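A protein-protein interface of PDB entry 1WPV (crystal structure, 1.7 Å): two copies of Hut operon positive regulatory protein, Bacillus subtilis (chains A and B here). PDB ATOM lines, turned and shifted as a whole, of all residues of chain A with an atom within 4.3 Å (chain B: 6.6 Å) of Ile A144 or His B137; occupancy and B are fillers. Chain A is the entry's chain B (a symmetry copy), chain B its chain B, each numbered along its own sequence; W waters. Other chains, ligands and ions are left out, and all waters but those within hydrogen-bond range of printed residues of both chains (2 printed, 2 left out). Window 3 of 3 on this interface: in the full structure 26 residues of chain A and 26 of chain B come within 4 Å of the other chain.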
ATOM      1  N   GLY A   9      -9.353  11.713  14.655  1.00  0.00           N
ATOM      2  CA  GLY A   9      -9.013  12.802  15.553  1.00  0.00           C
ATOM      3  C   GLY A   9      -8.669  14.080  14.807  1.00  0.00           C
ATOM      4  O   GLY A   9      -9.252  15.140  15.044  1.00  0.00           O
ATOM      5  N   GLU A  80     -12.596  12.280  28.208  1.00  0.00           N
ATOM      6  CA  GLU A  80     -11.217  12.395  27.767  1.00  0.00           C
ATOM      7  C   GLU A  80     -10.966  13.757  27.126  1.00  0.00           C
ATOM      8  O   GLU A  80      -9.934  14.382  27.361  1.00  0.00           O
ATOM      9  CB  GLU A  80     -10.869  11.243  26.810  1.00  0.00           C
ATOM     10  CG  GLU A  80     -10.821   9.892  27.526  1.00  0.00           C
ATOM     11  CD  GLU A  80     -10.092   8.816  26.736  1.00  0.00           C
ATOM     12  OE1 GLU A  80      -9.697   9.098  25.587  1.00  0.00           O
ATOM     13  N   TYR A 111      -9.128   3.008  11.009  1.00  0.00           N
ATOM     14  CA  TYR A 111      -8.083   2.025  10.715  1.00  0.00           C
ATOM     15  C   TYR A 111      -8.142   1.403   9.327  1.00  0.00           C
ATOM     16  O   TYR A 111      -9.180   1.407   8.668  1.00  0.00           O
ATOM     17  CB  TYR A 111      -8.104   0.903  11.765  1.00  0.00           C
ATOM     18  CG  TYR A 111      -7.863   1.405  13.165  1.00  0.00           C
ATOM     19  CD1 TYR A 111      -8.919   1.860  13.955  1.00  0.00           C
ATOM     20  CD2 TYR A 111      -6.568   1.527  13.662  1.00  0.00           C
ATOM     21  CE1 TYR A 111      -8.686   2.435  15.200  1.00  0.00           C
ATOM     22  CE2 TYR A 111      -6.325   2.100  14.904  1.00  0.00           C
ATOM     23  CZ  TYR A 111      -7.390   2.556  15.663  1.00  0.00           C
ATOM     24  OH  TYR A 111      -7.148   3.172  16.869  1.00  0.00           O
ATOM     25  N   TRP A 119     -15.263   3.878  15.678  1.00  0.00           N
ATOM     26  CA  TRP A 119     -14.618   4.563  16.782  1.00  0.00           C
ATOM     27  C   TRP A 119     -15.250   5.942  16.796  1.00  0.00           C
ATOM     28  O   TRP A 119     -15.883   6.349  15.823  1.00  0.00           O
ATOM     29  CB  TRP A 119     -13.109   4.679  16.559  1.00  0.00           C
ATOM     30  CG  TRP A 119     -12.407   3.386  16.743  1.00  0.00           C
ATOM     31  CD1 TRP A 119     -12.525   2.273  15.963  1.00  0.00           C
ATOM     32  CD2 TRP A 119     -11.511   3.043  17.803  1.00  0.00           C
ATOM     33  NE1 TRP A 119     -11.761   1.251  16.476  1.00  0.00           N
ATOM     34  CE2 TRP A 119     -11.128   1.697  17.607  1.00  0.00           C
ATOM     35  CE3 TRP A 119     -10.998   3.739  18.906  1.00  0.00           C
ATOM     36  CZ2 TRP A 119     -10.253   1.034  18.469  1.00  0.00           C
ATOM     37  CZ3 TRP A 119     -10.127   3.077  19.766  1.00  0.00           C
ATOM     38  CH2 TRP A 119      -9.767   1.739  19.540  1.00  0.00           C
ATOM     39  N   ILE A 120     -15.083   6.669  17.892  1.00  0.00           N
ATOM     40  CA  ILE A 120     -15.681   7.982  17.968  1.00  0.00           C
ATOM     41  C   ILE A 120     -14.687   8.971  18.552  1.00  0.00           C
ATOM     42  O   ILE A 120     -13.842   8.610  19.369  1.00  0.00           O
ATOM     43  CB  ILE A 120     -16.982   7.924  18.811  1.00  0.00           C
ATOM     44  CG1 ILE A 120     -17.795   9.202  18.624  1.00  0.00           C
ATOM     45  CG2 ILE A 120     -16.644   7.689  20.279  1.00  0.00           C
ATOM     46  CD1 ILE A 120     -19.182   9.135  19.266  1.00  0.00           C
ATOM     47  N   ALA A 121     -14.770  10.212  18.092  1.00  0.00           N
ATOM     48  CA  ALA A 121     -13.885  11.263  18.580  1.00  0.00           C
ATOM     49  C   ALA A 121     -14.707  12.465  19.008  1.00  0.00           C
ATOM     50  O   ALA A 121     -15.590  12.901  18.279  1.00  0.00           O
ATOM     51  CB  ALA A 121     -12.911  11.682  17.488  1.00  0.00           C
ATOM     52  N   VAL A 142      -9.404  16.610  23.003  1.00  0.00           N
ATOM     53  CA  VAL A 142      -9.822  15.556  22.079  1.00  0.00           C
ATOM     54  C   VAL A 142      -9.856  14.209  22.792  1.00  0.00           C
ATOM     55  O   VAL A 142      -8.878  13.806  23.429  1.00  0.00           O
ATOM     56  CB  VAL A 142      -8.879  15.439  20.856  1.00  0.00           C
ATOM     57  CG1 VAL A 142      -9.307  14.262  19.975  1.00  0.00           C
ATOM     58  CG2 VAL A 142      -8.913  16.713  20.059  1.00  0.00           C
ATOM     59  N   GLY A 143     -10.997  13.532  22.690  1.00  0.00           N
ATOM     60  CA  GLY A 143     -11.167  12.229  23.308  1.00  0.00           C
ATOM     61  C   GLY A 143     -11.522  11.228  22.227  1.00  0.00           C
ATOM     62  O   GLY A 143     -12.354  11.516  21.367  1.00  0.00           O
ATOM     63  N   ILE A 144     -10.892  10.059  22.263  1.00  0.00           N
ATOM     64  CA  ILE A 144     -11.148   9.031  21.254  1.00  0.00           C
ATOM     65  C   ILE A 144     -11.508   7.711  21.931  1.00  0.00           C
ATOM     66  O   ILE A 144     -10.882   7.319  22.913  1.00  0.00           O
ATOM     67  CB  ILE A 144      -9.904   8.874  20.333  1.00  0.00           C
ATOM     68  CG1 ILE A 144      -9.799  10.116  19.428  1.00  0.00           C
ATOM     69  CG2 ILE A 144     -10.009   7.602  19.498  1.00  0.00           C
ATOM     70  CD1 ILE A 144      -8.546  10.204  18.589  1.00  0.00           C
ATOM     71  N   ASN A 145     -12.528   7.030  21.409  1.00  0.00           N
ATOM     72  CA  ASN A 145     -12.972   5.781  22.006  1.00  0.00           C
ATOM     73  C   ASN A 145     -13.549   4.848  20.950  1.00  0.00           C
ATOM     74  O   ASN A 145     -13.956   5.298  19.882  1.00  0.00           O
ATOM     75  CB  ASN A 145     -14.045   6.082  23.063  1.00  0.00           C
ATOM     76  CG  ASN A 145     -14.132   5.016  24.147  1.00  0.00           C
ATOM     77  OD1 ASN A 145     -13.336   4.081  24.180  1.00  0.00           O
ATOM     78  ND2 ASN A 145     -15.104   5.166  25.055  1.00  0.00           N
ATOM     79  N   ARG B  87      -4.524  12.481  29.508  1.00  0.00           N
ATOM     80  CA  ARG B  87      -5.884  12.355  30.044  1.00  0.00           C
ATOM     81  C   ARG B  87      -6.047  11.696  31.414  1.00  0.00           C
ATOM     82  O   ARG B  87      -6.737  10.680  31.543  1.00  0.00           O
ATOM     83  CB  ARG B  87      -6.768  11.611  29.028  1.00  0.00           C
ATOM     84  CG  ARG B  87      -7.101  12.419  27.773  1.00  0.00           C
ATOM     85  CD  ARG B  87      -7.149  11.539  26.537  1.00  0.00           C
ATOM     86  NE  ARG B  87      -5.840  10.931  26.291  1.00  0.00           N
ATOM     87  CZ  ARG B  87      -5.629   9.622  26.170  1.00  0.00           C
ATOM     88  NH1 ARG B  87      -6.646   8.766  26.256  1.00  0.00           N
ATOM     89  NH2 ARG B  87      -4.390   9.166  26.012  1.00  0.00           N
ATOM     90  N   GLY B 126      -0.363  13.429  17.704  1.00  0.00           N
ATOM     91  CA  GLY B 126       0.265  12.210  17.247  1.00  0.00           C
ATOM     92  C   GLY B 126      -0.542  11.026  17.710  1.00  0.00           C
ATOM     93  O   GLY B 126      -1.774  11.054  17.716  1.00  0.00           O
ATOM     94  N   THR B 127       0.152   9.976  18.109  1.00  0.00           N
ATOM     95  CA  THR B 127      -0.529   8.784  18.567  1.00  0.00           C
ATOM     96  C   THR B 127      -0.057   8.413  19.952  1.00  0.00           C
ATOM     97  O   THR B 127       1.020   8.823  20.394  1.00  0.00           O
ATOM     98  CB  THR B 127      -0.225   7.574  17.669  1.00  0.00           C
ATOM     99  OG1 THR B 127       1.186   7.323  17.695  1.00  0.00           O
ATOM    100  CG2 THR B 127      -0.676   7.824  16.239  1.00  0.00           C
ATOM    101  N   ILE B 128      -0.896   7.645  20.630  1.00  0.00           N
ATOM    102  CA  ILE B 128      -0.592   7.122  21.943  1.00  0.00           C
ATOM    103  C   ILE B 128      -1.119   5.693  21.851  1.00  0.00           C
ATOM    104  O   ILE B 128      -2.188   5.458  21.289  1.00  0.00           O
ATOM    105  CB  ILE B 128      -1.296   7.923  23.071  1.00  0.00           C
ATOM    106  CG1 ILE B 128      -0.790   7.426  24.427  1.00  0.00           C
ATOM    107  CG2 ILE B 128      -2.813   7.768  22.976  1.00  0.00           C
ATOM    108  CD1 ILE B 128      -1.046   8.372  25.580  1.00  0.00           C
ATOM    109  N   GLY B 129      -0.353   4.731  22.354  1.00  0.00           N
ATOM    110  CA  GLY B 129      -0.795   3.357  22.272  1.00  0.00           C
ATOM    111  C   GLY B 129       0.174   2.389  22.911  1.00  0.00           C
ATOM    112  O   GLY B 129       1.092   2.784  23.614  1.00  0.00           O
ATOM    113  N   GLY B 134       0.681  -0.430  15.831  1.00  0.00           N
ATOM    114  CA  GLY B 134      -0.582  -0.784  15.223  1.00  0.00           C
ATOM    115  C   GLY B 134      -1.683  -0.618  16.245  1.00  0.00           C
ATOM    116  O   GLY B 134      -2.816  -0.251  15.920  1.00  0.00           O
ATOM    117  N   LEU B 135      -1.325  -0.874  17.498  1.00  0.00           N
ATOM    118  CA  LEU B 135      -2.253  -0.763  18.615  1.00  0.00           C
ATOM    119  C   LEU B 135      -2.189   0.637  19.206  1.00  0.00           C
ATOM    120  O   LEU B 135      -1.575   0.859  20.247  1.00  0.00           O
ATOM    121  CB  LEU B 135      -1.905  -1.789  19.696  1.00  0.00           C
ATOM    122  CG  LEU B 135      -1.831  -3.267  19.295  1.00  0.00           C
ATOM    123  CD1 LEU B 135      -1.598  -4.104  20.541  1.00  0.00           C
ATOM    124  CD2 LEU B 135      -3.108  -3.695  18.601  1.00  0.00           C
ATOM    125  N   GLU B 136      -2.843   1.584  18.551  1.00  0.00           N
ATOM    126  CA  GLU B 136      -2.806   2.949  19.043  1.00  0.00           C
ATOM    127  C   GLU B 136      -3.891   3.800  18.397  1.00  0.00           C
ATOM    128  O   GLU B 136      -4.518   3.392  17.426  1.00  0.00           O
ATOM    129  CB  GLU B 136      -1.452   3.554  18.692  1.00  0.00           C
ATOM    130  CG  GLU B 136      -1.330   3.872  17.192  1.00  0.00           C
ATOM    131  CD  GLU B 136       0.011   3.489  16.587  1.00  0.00           C
ATOM    132  OE1 GLU B 136       0.778   2.740  17.230  1.00  0.00           O
ATOM    133  OE2 GLU B 136       0.290   3.933  15.451  1.00  0.00           O
ATOM    134  N   HIS B 137      -4.115   4.977  18.966  1.00  0.00           N
ATOM    135  CA  HIS B 137      -5.049   5.934  18.389  1.00  0.00           C
ATOM    136  C   HIS B 137      -4.431   7.320  18.559  1.00  0.00           C
ATOM    137  O   HIS B 137      -3.365   7.463  19.163  1.00  0.00           O
ATOM    138  CB  HIS B 137      -6.452   5.838  19.023  1.00  0.00           C
ATOM    139  CG  HIS B 137      -6.495   6.109  20.490  1.00  0.00           C
ATOM    140  ND1 HIS B 137      -6.224   7.346  21.030  1.00  0.00           N
ATOM    141  CD2 HIS B 137      -6.815   5.304  21.530  1.00  0.00           C
ATOM    142  CE1 HIS B 137      -6.372   7.293  22.342  1.00  0.00           C
ATOM    143  NE2 HIS B 137      -6.731   6.067  22.670  1.00  0.00           N
ATOM    144  N   GLU B 138      -5.084   8.336  18.003  1.00  0.00           N
ATOM    145  CA  GLU B 138      -4.578   9.697  18.062  1.00  0.00           C
ATOM    146  C   GLU B 138      -4.661  10.304  19.443  1.00  0.00           C
ATOM    147  O   GLU B 138      -5.436   9.860  20.295  1.00  0.00           O
ATOM    148  CB  GLU B 138      -5.346  10.571  17.075  1.00  0.00           C
ATOM    149  CG  GLU B 138      -5.121  10.185  15.633  1.00  0.00           C
ATOM    150  CD  GLU B 138      -6.249  10.644  14.747  1.00  0.00           C
ATOM    151  OE1 GLU B 138      -7.281   9.936  14.692  1.00  0.00           O
ATOM    152  OE2 GLU B 138      -6.110  11.716  14.127  1.00  0.00           O
ATOM    153  N   THR B 139      -3.854  11.337  19.647  1.00  0.00           N
ATOM    154  CA  THR B 139      -3.807  12.042  20.913  1.00  0.00           C
ATOM    155  C   THR B 139      -3.481  13.505  20.608  1.00  0.00           C
ATOM    156  O   THR B 139      -2.771  13.793  19.648  1.00  0.00           O
ATOM    157  CB  THR B 139      -2.735  11.419  21.830  1.00  0.00           C
ATOM    158  OG1 THR B 139      -2.937  11.873  23.170  1.00  0.00           O
ATOM    159  CG2 THR B 139      -1.328  11.790  21.356  1.00  0.00           C
ATOM    160  N   PHE B 140      -4.023  14.417  21.413  1.00  0.00           N
ATOM    161  CA  PHE B 140      -3.836  15.858  21.235  1.00  0.00           C
ATOM    162  C   PHE B 140      -3.665  16.552  22.576  1.00  0.00           C
ATOM    163  O   PHE B 140      -4.139  16.069  23.604  1.00  0.00           O
ATOM    164  CB  PHE B 140      -5.073  16.522  20.626  1.00  0.00           C
ATOM    165  CG  PHE B 140      -5.212  16.395  19.147  1.00  0.00           C
ATOM    166  CD1 PHE B 140      -5.826  15.280  18.585  1.00  0.00           C
ATOM    167  CD2 PHE B 140      -4.860  17.464  18.320  1.00  0.00           C
ATOM    168  CE1 PHE B 140      -6.106  15.231  17.225  1.00  0.00           C
ATOM    169  CE2 PHE B 140      -5.133  17.426  16.954  1.00  0.00           C
ATOM    170  CZ  PHE B 140      -5.762  16.308  16.406  1.00  0.00           C
HETATM  171  O   HOH W   1      -6.102  13.451  23.382  1.00  0.00           O
HETATM  172  O   HOH W   2      -6.772  16.859  24.150  1.00  0.00           O
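The guanidinium group (NH1) of Arg B87 is in salt-bridge range of the side-chain carboxylate (OE1) of Glu A80 (3.1 Å). The backbone carbonyl oxygen (O) of Glu B136 is in hydrogen-bond range of the side-chain hydroxyl (OH) of Tyr A111, 2.7 Å away. The side-chain carboxylate (OE1) of Glu B138 lies within hydrogen-bond range of the backbone NH (N) of Gly A9, at 2.7 Å.
The backbone carbonyl oxygen (O) of His B137 is in hydrogen-bond range of the backbone NH (N) of Ile B128, 2.9 Å away. The backbone NH (N) of Gly B134 is in hydrogen-bond range of the side-chain carboxylate (OE1) of Glu B136 (3.5 Å).
Among the printed residues, merely in contact across the chains: Gly A9 with Phe B140, Tyr A111 with His B137, Val A142 with Phe B140, Ile A144 with His B137 and Ile A144 with Glu B138.
Of the printed residues of chain B, Glu A80 touches Arg B87. Printed residues of chain B within 4 Å of Tyr A111: Glu B136 (2.7 Å) and His B137 (3.5 Å). Of the printed residues of chain B, Val A142 touches Phe B140. Of the printed residues of chain B, Ile A144 touches His B137 (3.9 Å) and Glu B138 (3.6 Å). Gly B134 touches none of the printed residues of chain A. Of the printed residues of chain A, His B137 touches Tyr A111 and Ile A144. Of the printed residues of chain A, Glu B138 touches Gly A9 and Ile A144. The nearest residue of chain B that does not touch Ile A144 is Thr B139 (4.9 Å).
Hydrophobic or aromatic side chains of chain A within 4 Å of the printed part of chain B: Tyr A111, Val A142 and Ile A144. Of the 12 printed residues of chain B, 5 touch a printed residue of chain A. Printed residues of chain B that touch a printed residue of chain A: Arg B87, Glu B136, His B137, Glu B138 and Phe B140. Among the printed residues, 8 pairs touch across the chains.
No position is printed for both chains. Of the 8 pairs that touch across the chains among the printed residues, none has its exchanged pair printed and touching as well.
Water W1 lies within hydrogen-bond range of the backbone carbonyl oxygen (O) of Val A142 (2.8 Å) and the backbone NH (N) of Phe B140 (3.0 Å). Water W2 lies within hydrogen-bond range of O of Phe B140 and N of Val A142.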
